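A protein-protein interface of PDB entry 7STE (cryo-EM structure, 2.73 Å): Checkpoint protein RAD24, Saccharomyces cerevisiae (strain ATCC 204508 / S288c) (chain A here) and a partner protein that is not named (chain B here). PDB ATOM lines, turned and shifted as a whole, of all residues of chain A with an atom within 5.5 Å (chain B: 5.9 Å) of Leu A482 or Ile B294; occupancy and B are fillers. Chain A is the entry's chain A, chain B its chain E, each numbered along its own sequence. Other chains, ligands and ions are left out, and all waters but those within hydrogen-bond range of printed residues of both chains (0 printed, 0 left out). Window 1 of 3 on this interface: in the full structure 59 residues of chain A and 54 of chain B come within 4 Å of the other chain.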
ATOM      1  N   PHE A 477      -1.542 -24.849  21.486  1.00  0.00           N
ATOM      2  CA  PHE A 477      -1.462 -25.850  22.544  1.00  0.00           C
ATOM      3  C   PHE A 477      -2.779 -25.955  23.305  1.00  0.00           C
ATOM      4  O   PHE A 477      -3.217 -27.058  23.653  1.00  0.00           O
ATOM      5  CB  PHE A 477      -0.317 -25.512  23.498  1.00  0.00           C
ATOM      6  CG  PHE A 477      -0.186 -26.468  24.649  1.00  0.00           C
ATOM      7  CD1 PHE A 477       0.297 -27.750  24.450  1.00  0.00           C
ATOM      8  CD2 PHE A 477      -0.543 -26.084  25.930  1.00  0.00           C
ATOM      9  CE1 PHE A 477       0.419 -28.632  25.507  1.00  0.00           C
ATOM     10  CE2 PHE A 477      -0.423 -26.961  26.991  1.00  0.00           C
ATOM     11  CZ  PHE A 477       0.059 -28.236  26.778  1.00  0.00           C
ATOM     12  N   ARG A 478      -3.419 -24.816  23.583  1.00  0.00           N
ATOM     13  CA  ARG A 478      -4.688 -24.844  24.304  1.00  0.00           C
ATOM     14  C   ARG A 478      -5.749 -25.610  23.525  1.00  0.00           C
ATOM     15  O   ARG A 478      -6.506 -26.398  24.102  1.00  0.00           O
ATOM     16  CB  ARG A 478      -5.161 -23.419  24.591  1.00  0.00           C
ATOM     17  CG  ARG A 478      -4.346 -22.699  25.651  1.00  0.00           C
ATOM     18  CD  ARG A 478      -4.851 -21.285  25.871  1.00  0.00           C
ATOM     19  NE  ARG A 478      -6.191 -21.264  26.447  1.00  0.00           N
ATOM     20  CZ  ARG A 478      -6.452 -21.298  27.747  1.00  0.00           C
ATOM     21  NH1 ARG A 478      -5.486 -21.368  28.649  1.00  0.00           N
ATOM     22  NH2 ARG A 478      -7.719 -21.263  28.155  1.00  0.00           N
ATOM     23  N   ASN A 479      -5.820 -25.389  22.211  1.00  0.00           N
ATOM     24  CA  ASN A 479      -6.787 -26.118  21.397  1.00  0.00           C
ATOM     25  C   ASN A 479      -6.504 -27.614  21.420  1.00  0.00           C
ATOM     26  O   ASN A 479      -7.432 -28.430  21.475  1.00  0.00           O
ATOM     27  CB  ASN A 479      -6.769 -25.589  19.963  1.00  0.00           C
ATOM     28  CG  ASN A 479      -7.232 -24.149  19.867  1.00  0.00           C
ATOM     29  OD1 ASN A 479      -7.890 -23.635  20.772  1.00  0.00           O
ATOM     30  ND2 ASN A 479      -6.891 -23.490  18.767  1.00  0.00           N
ATOM     31  N   ILE A 480      -5.226 -27.996  21.379  1.00  0.00           N
ATOM     32  CA  ILE A 480      -4.872 -29.410  21.442  1.00  0.00           C
ATOM     33  C   ILE A 480      -5.314 -30.007  22.772  1.00  0.00           C
ATOM     34  O   ILE A 480      -5.883 -31.105  22.819  1.00  0.00           O
ATOM     35  CB  ILE A 480      -3.361 -29.594  21.214  1.00  0.00           C
ATOM     36  CG1 ILE A 480      -2.987 -29.187  19.787  1.00  0.00           C
ATOM     37  CG2 ILE A 480      -2.954 -31.037  21.482  1.00  0.00           C
ATOM     38  CD1 ILE A 480      -1.502 -28.975  19.577  1.00  0.00           C
ATOM     39  N   THR A 481      -5.061 -29.296  23.872  1.00  0.00           N
ATOM     40  CA  THR A 481      -5.445 -29.808  25.184  1.00  0.00           C
ATOM     41  C   THR A 481      -6.959 -29.928  25.309  1.00  0.00           C
ATOM     42  O   THR A 481      -7.466 -30.890  25.898  1.00  0.00           O
ATOM     43  CB  THR A 481      -4.894 -28.905  26.287  1.00  0.00           C
ATOM     44  OG1 THR A 481      -5.360 -27.565  26.092  1.00  0.00           O
ATOM     45  CG2 THR A 481      -3.371 -28.919  26.289  1.00  0.00           C
ATOM     46  N   LEU A 482      -7.697 -28.961  24.764  1.00  0.00           N
ATOM     47  CA  LEU A 482      -9.138 -28.898  24.972  1.00  0.00           C
ATOM     48  C   LEU A 482      -9.934 -29.601  23.877  1.00  0.00           C
ATOM     49  O   LEU A 482     -10.896 -30.315  24.181  1.00  0.00           O
ATOM     50  CB  LEU A 482      -9.587 -27.437  25.068  1.00  0.00           C
ATOM     51  CG  LEU A 482      -8.994 -26.619  26.217  1.00  0.00           C
ATOM     52  CD1 LEU A 482      -9.512 -25.191  26.175  1.00  0.00           C
ATOM     53  CD2 LEU A 482      -9.301 -27.261  27.563  1.00  0.00           C
ATOM     54  N   GLU A 483      -9.562 -29.419  22.609  1.00  0.00           N
ATOM     55  CA  GLU A 483     -10.384 -29.870  21.492  1.00  0.00           C
ATOM     56  C   GLU A 483      -9.734 -30.995  20.696  1.00  0.00           C
ATOM     57  O   GLU A 483     -10.322 -32.071  20.560  1.00  0.00           O
ATOM     58  CB  GLU A 483     -10.694 -28.680  20.573  1.00  0.00           C
ATOM     59  CG  GLU A 483     -11.407 -27.533  21.273  1.00  0.00           C
ATOM     60  CD  GLU A 483     -11.391 -26.255  20.459  1.00  0.00           C
ATOM     61  OE1 GLU A 483     -11.296 -26.341  19.217  1.00  0.00           O
ATOM     62  OE2 GLU A 483     -11.472 -25.165  21.061  1.00  0.00           O
ATOM     63  N   PHE A 484      -8.530 -30.780  20.163  1.00  0.00           N
ATOM     64  CA  PHE A 484      -7.903 -31.780  19.308  1.00  0.00           C
ATOM     65  C   PHE A 484      -7.260 -32.915  20.092  1.00  0.00           C
ATOM     66  O   PHE A 484      -6.845 -33.907  19.484  1.00  0.00           O
ATOM     67  CB  PHE A 484      -6.851 -31.123  18.409  1.00  0.00           C
ATOM     68  CG  PHE A 484      -7.422 -30.142  17.427  1.00  0.00           C
ATOM     69  CD1 PHE A 484      -7.945 -30.576  16.220  1.00  0.00           C
ATOM     70  CD2 PHE A 484      -7.434 -28.788  17.709  1.00  0.00           C
ATOM     71  CE1 PHE A 484      -8.469 -29.675  15.314  1.00  0.00           C
ATOM     72  CE2 PHE A 484      -7.959 -27.883  16.808  1.00  0.00           C
ATOM     73  CZ  PHE A 484      -8.476 -28.327  15.609  1.00  0.00           C
ATOM     74  N   GLY A 485      -7.166 -32.798  21.418  1.00  0.00           N
ATOM     75  CA  GLY A 485      -6.601 -33.878  22.207  1.00  0.00           C
ATOM     76  C   GLY A 485      -7.429 -35.145  22.156  1.00  0.00           C
ATOM     77  O   GLY A 485      -6.885 -36.250  22.230  1.00  0.00           O
ATOM     78  N   ARG A 538      -5.825 -41.249  22.405  1.00  0.00           N
ATOM     79  CA  ARG A 538      -6.026 -39.946  23.023  1.00  0.00           C
ATOM     80  C   ARG A 538      -4.742 -39.486  23.701  1.00  0.00           C
ATOM     81  O   ARG A 538      -4.100 -40.249  24.429  1.00  0.00           O
ATOM     82  CB  ARG A 538      -7.169 -40.016  24.035  1.00  0.00           C
ATOM     83  CG  ARG A 538      -7.682 -38.661  24.494  1.00  0.00           C
ATOM     84  CD  ARG A 538      -7.207 -38.330  25.898  1.00  0.00           C
ATOM     85  NE  ARG A 538      -7.670 -37.019  26.337  1.00  0.00           N
ATOM     86  CZ  ARG A 538      -7.088 -35.869  26.019  1.00  0.00           C
ATOM     87  NH1 ARG A 538      -6.010 -35.828  25.253  1.00  0.00           N
ATOM     88  NH2 ARG A 538      -7.603 -34.733  26.480  1.00  0.00           N
ATOM     89  N   ASN B  45     -13.567 -17.595  21.780  1.00  0.00           N
ATOM     90  CA  ASN B  45     -12.739 -18.605  21.139  1.00  0.00           C
ATOM     91  C   ASN B  45     -13.551 -19.405  20.127  1.00  0.00           C
ATOM     92  O   ASN B  45     -14.734 -19.684  20.334  1.00  0.00           O
ATOM     93  CB  ASN B  45     -12.144 -19.543  22.189  1.00  0.00           C
ATOM     94  CG  ASN B  45     -11.112 -20.489  21.609  1.00  0.00           C
ATOM     95  OD1 ASN B  45     -10.845 -20.475  20.408  1.00  0.00           O
ATOM     96  ND2 ASN B  45     -10.527 -21.321  22.462  1.00  0.00           N
ATOM     97  N   PRO B 257     -16.710 -33.299  24.422  1.00  0.00           N
ATOM     98  CA  PRO B 257     -15.347 -33.543  24.907  1.00  0.00           C
ATOM     99  C   PRO B 257     -15.350 -34.457  26.124  1.00  0.00           C
ATOM    100  O   PRO B 257     -16.230 -34.379  26.983  1.00  0.00           O
ATOM    101  CB  PRO B 257     -14.834 -32.141  25.252  1.00  0.00           C
ATOM    102  CG  PRO B 257     -15.668 -31.217  24.434  1.00  0.00           C
ATOM    103  CD  PRO B 257     -17.017 -31.860  24.344  1.00  0.00           C
ATOM    104  N   ASP B 258     -14.345 -35.333  26.190  1.00  0.00           N
ATOM    105  CA  ASP B 258     -14.285 -36.308  27.274  1.00  0.00           C
ATOM    106  C   ASP B 258     -14.160 -35.623  28.630  1.00  0.00           C
ATOM    107  O   ASP B 258     -14.811 -36.028  29.601  1.00  0.00           O
ATOM    108  CB  ASP B 258     -13.118 -37.270  27.048  1.00  0.00           C
ATOM    109  CG  ASP B 258     -11.791 -36.552  26.899  1.00  0.00           C
ATOM    110  OD1 ASP B 258     -11.798 -35.351  26.558  1.00  0.00           O
ATOM    111  OD2 ASP B 258     -10.741 -37.191  27.119  1.00  0.00           O
ATOM    112  N   TRP B 259     -13.326 -34.585  28.719  1.00  0.00           N
ATOM    113  CA  TRP B 259     -13.165 -33.885  29.989  1.00  0.00           C
ATOM    114  C   TRP B 259     -14.456 -33.198  30.417  1.00  0.00           C
ATOM    115  O   TRP B 259     -14.728 -33.090  31.618  1.00  0.00           O
ATOM    116  CB  TRP B 259     -12.019 -32.876  29.894  1.00  0.00           C
ATOM    117  CG  TRP B 259     -12.239 -31.775  28.900  1.00  0.00           C
ATOM    118  CD1 TRP B 259     -12.175 -31.870  27.540  1.00  0.00           C
ATOM    119  CD2 TRP B 259     -12.543 -30.406  29.191  1.00  0.00           C
ATOM    120  NE1 TRP B 259     -12.427 -30.648  26.968  1.00  0.00           N
ATOM    121  CE2 TRP B 259     -12.656 -29.732  27.960  1.00  0.00           C
ATOM    122  CE3 TRP B 259     -12.734 -29.687  30.375  1.00  0.00           C
ATOM    123  CZ2 TRP B 259     -12.953 -28.374  27.878  1.00  0.00           C
ATOM    124  CZ3 TRP B 259     -13.028 -28.339  30.291  1.00  0.00           C
ATOM    125  CH2 TRP B 259     -13.135 -27.696  29.051  1.00  0.00           C
ATOM    126  N   LEU B 289      -7.671 -34.703  35.841  1.00  0.00           N
ATOM    127  CA  LEU B 289      -7.961 -33.658  34.864  1.00  0.00           C
ATOM    128  C   LEU B 289      -6.763 -32.738  34.665  1.00  0.00           C
ATOM    129  O   LEU B 289      -6.440 -32.364  33.531  1.00  0.00           O
ATOM    130  CB  LEU B 289      -9.185 -32.854  35.305  1.00  0.00           C
ATOM    131  CG  LEU B 289     -10.549 -33.454  34.961  1.00  0.00           C
ATOM    132  CD1 LEU B 289     -11.657 -32.707  35.683  1.00  0.00           C
ATOM    133  CD2 LEU B 289     -10.784 -33.431  33.459  1.00  0.00           C
ATOM    134  N   LEU B 290      -6.095 -32.357  35.756  1.00  0.00           N
ATOM    135  CA  LEU B 290      -4.949 -31.459  35.648  1.00  0.00           C
ATOM    136  C   LEU B 290      -3.785 -32.115  34.919  1.00  0.00           C
ATOM    137  O   LEU B 290      -3.035 -31.433  34.211  1.00  0.00           O
ATOM    138  CB  LEU B 290      -4.509 -31.001  37.038  1.00  0.00           C
ATOM    139  CG  LEU B 290      -5.387 -29.937  37.701  1.00  0.00           C
ATOM    140  CD1 LEU B 290      -5.080 -29.845  39.186  1.00  0.00           C
ATOM    141  CD2 LEU B 290      -5.197 -28.585  37.030  1.00  0.00           C
ATOM    142  N   ALA B 291      -3.616 -33.429  35.077  1.00  0.00           N
ATOM    143  CA  ALA B 291      -2.516 -34.121  34.417  1.00  0.00           C
ATOM    144  C   ALA B 291      -2.606 -34.030  32.900  1.00  0.00           C
ATOM    145  O   ALA B 291      -1.596 -34.233  32.217  1.00  0.00           O
ATOM    146  CB  ALA B 291      -2.485 -35.589  34.847  1.00  0.00           C
ATOM    147  N   HIS B 292      -3.785 -33.729  32.358  1.00  0.00           N
ATOM    148  CA  HIS B 292      -3.977 -33.587  30.923  1.00  0.00           C
ATOM    149  C   HIS B 292      -3.824 -32.142  30.455  1.00  0.00           C
ATOM    150  O   HIS B 292      -4.249 -31.809  29.342  1.00  0.00           O
ATOM    151  CB  HIS B 292      -5.349 -34.137  30.524  1.00  0.00           C
ATOM    152  CG  HIS B 292      -5.357 -35.615  30.288  1.00  0.00           C
ATOM    153  ND1 HIS B 292      -5.318 -36.533  31.315  1.00  0.00           N
ATOM    154  CD2 HIS B 292      -5.397 -36.335  29.142  1.00  0.00           C
ATOM    155  CE1 HIS B 292      -5.332 -37.755  30.813  1.00  0.00           C
ATOM    156  NE2 HIS B 292      -5.381 -37.663  29.496  1.00  0.00           N
ATOM    157  N   CYS B 293      -3.231 -31.282  31.283  1.00  0.00           N
ATOM    158  CA  CYS B 293      -2.935 -29.892  30.946  1.00  0.00           C
ATOM    159  C   CYS B 293      -4.188 -29.046  30.766  1.00  0.00           C
ATOM    160  O   CYS B 293      -4.156 -28.033  30.060  1.00  0.00           O
ATOM    161  CB  CYS B 293      -2.065 -29.804  29.686  1.00  0.00           C
ATOM    162  SG  CYS B 293      -0.482 -30.667  29.822  1.00  0.00           S
ATOM    163  N   ILE B 294      -5.297 -29.432  31.390  1.00  0.00           N
ATOM    164  CA  ILE B 294      -6.516 -28.629  31.359  1.00  0.00           C
ATOM    165  C   ILE B 294      -6.340 -27.475  32.342  1.00  0.00           C
ATOM    166  O   ILE B 294      -6.038 -27.717  33.519  1.00  0.00           O
ATOM    167  CB  ILE B 294      -7.757 -29.469  31.703  1.00  0.00           C
ATOM    168  CG1 ILE B 294      -7.803 -30.745  30.855  1.00  0.00           C
ATOM    169  CG2 ILE B 294      -9.023 -28.649  31.501  1.00  0.00           C
ATOM    170  CD1 ILE B 294      -7.976 -30.502  29.366  1.00  0.00           C
ATOM    171  N   PRO B 295      -6.506 -26.220  31.922  1.00  0.00           N
ATOM    172  CA  PRO B 295      -6.303 -25.106  32.859  1.00  0.00           C
ATOM    173  C   PRO B 295      -7.239 -25.201  34.055  1.00  0.00           C
ATOM    174  O   PRO B 295      -8.391 -25.624  33.938  1.00  0.00           O
ATOM    175  CB  PRO B 295      -6.599 -23.865  32.009  1.00  0.00           C
ATOM    176  CG  PRO B 295      -6.416 -24.304  30.602  1.00  0.00           C
ATOM    177  CD  PRO B 295      -6.821 -25.742  30.564  1.00  0.00           C
ATOM    178  N   ALA B 296      -6.726 -24.793  35.219  1.00  0.00           N
ATOM    179  CA  ALA B 296      -7.521 -24.856  36.442  1.00  0.00           C
ATOM    180  C   ALA B 296      -8.739 -23.946  36.359  1.00  0.00           C
ATOM    181  O   ALA B 296      -9.830 -24.313  36.813  1.00  0.00           O
ATOM    182  CB  ALA B 296      -6.655 -24.483  37.646  1.00  0.00           C
ATOM    183  N   ILE B 298     -10.428 -23.054  33.705  1.00  0.00           N
ATOM    184  CA  ILE B 298     -11.426 -23.677  32.839  1.00  0.00           C
ATOM    185  C   ILE B 298     -12.173 -24.770  33.593  1.00  0.00           C
ATOM    186  O   ILE B 298     -13.398 -24.895  33.483  1.00  0.00           O
ATOM    187  CB  ILE B 298     -10.759 -24.224  31.564  1.00  0.00           C
ATOM    188  CG1 ILE B 298     -10.097 -23.091  30.769  1.00  0.00           C
ATOM    189  CG2 ILE B 298     -11.775 -24.960  30.702  1.00  0.00           C
ATOM    190  CD1 ILE B 298     -11.052 -22.004  30.310  1.00  0.00           C
ATOM    191  N   ILE B 299     -11.445 -25.583  34.363  1.00  0.00           N
ATOM    192  CA  ILE B 299     -12.088 -26.637  35.141  1.00  0.00           C
ATOM    193  C   ILE B 299     -13.070 -26.034  36.134  1.00  0.00           C
ATOM    194  O   ILE B 299     -14.200 -26.516  36.284  1.00  0.00           O
ATOM    195  CB  ILE B 299     -11.030 -27.500  35.854  1.00  0.00           C
ATOM    196  CG1 ILE B 299     -10.126 -28.195  34.835  1.00  0.00           C
ATOM    197  CG2 ILE B 299     -11.704 -28.528  36.756  1.00  0.00           C
ATOM    198  CD1 ILE B 299      -8.865 -28.781  35.435  1.00  0.00           C
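The guanidinium group of Arg A538 lies within salt-bridge range of the side-chain carboxylate of Asp B258 (3.2 Å). The backbone carbonyl oxygen (O) of Leu A482 sits at hydrogen-bond distance from the indole nitrogen (NE1) of Trp B259 (3.2 Å).
The backbone carbonyl oxygen (O) of Asn A479 is in hydrogen-bond range of the backbone NH (N) of Phe A484, at 2.9 Å. The backbone carbonyl oxygen (O) of Phe A477 sits close to the side-chain hydroxyl (OG1) of Thr A481, at 3.3 Å. O of Gly A485 is in hydrogen-bond range of NH1 of Arg A538, at 3.2 Å. O of Arg A478 lies within hydrogen-bond range of OG1 of Thr A481 (2.6 Å).
CB of Cys B293 touches CZ of Phe A477, 3.9 Å away. CG of Pro B295 touches NH1 of Arg A478, 3.6 Å away. Arg A478 touches Ile B298. OD1 of Asn A479 touches ND2 of Asn B45, at 3.9 Å. Cys B293 touches Thr A481 (CB to CG2, 3.7 Å). Ile B294 touches Thr A481. Leu A482 touches Ile B294 (CD2 to CD1, 3.9 Å). CD2 of His B292 touches CZ of Arg A538, at 3.6 Å.
Ile A480 touches none of the printed residues of chain B. Leu A482 touches just these residues of chain B: Trp B259 (3.2 Å) and Ile B294 (3.9 Å). Gly A485 touches none of the printed residues of chain B. Of the printed residues of chain B, Arg A538 touches Asp B258 and His B292. Of the printed residues of chain A, His B292 touches Arg A538 (3.6 Å). Printed residues of chain A within 4 Å of Cys B293: Phe A477 and Thr A481. Of chain A, only Thr A481 (3.5 Å) and Leu A482 (3.9 Å) come within 4 Å of Ile B294. Printed residues of chain A within 4 Å of Pro B295: Arg A478 (3.6 Å).
Of the 14 printed residues of chain B, 8 touch a printed residue of chain A. Hydrophobic or aromatic side chains of chain B that line the printed part of chain A: Trp B259, His B292, Ile B294, Pro B295 and Ile B298. Printed residues of chain A that touch a printed residue of chain B: Phe A477, Arg A478, Asn A479, Thr A481, Leu A482 and Arg A538. Among the printed residues, 10 pairs touch across the chains. Among the printed residues, Asp or Glu carboxylates within 4 Å of a Lys or Arg side-chain nitrogen of the other chain: Arg A538 with Asp B258 (3.2 Å).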
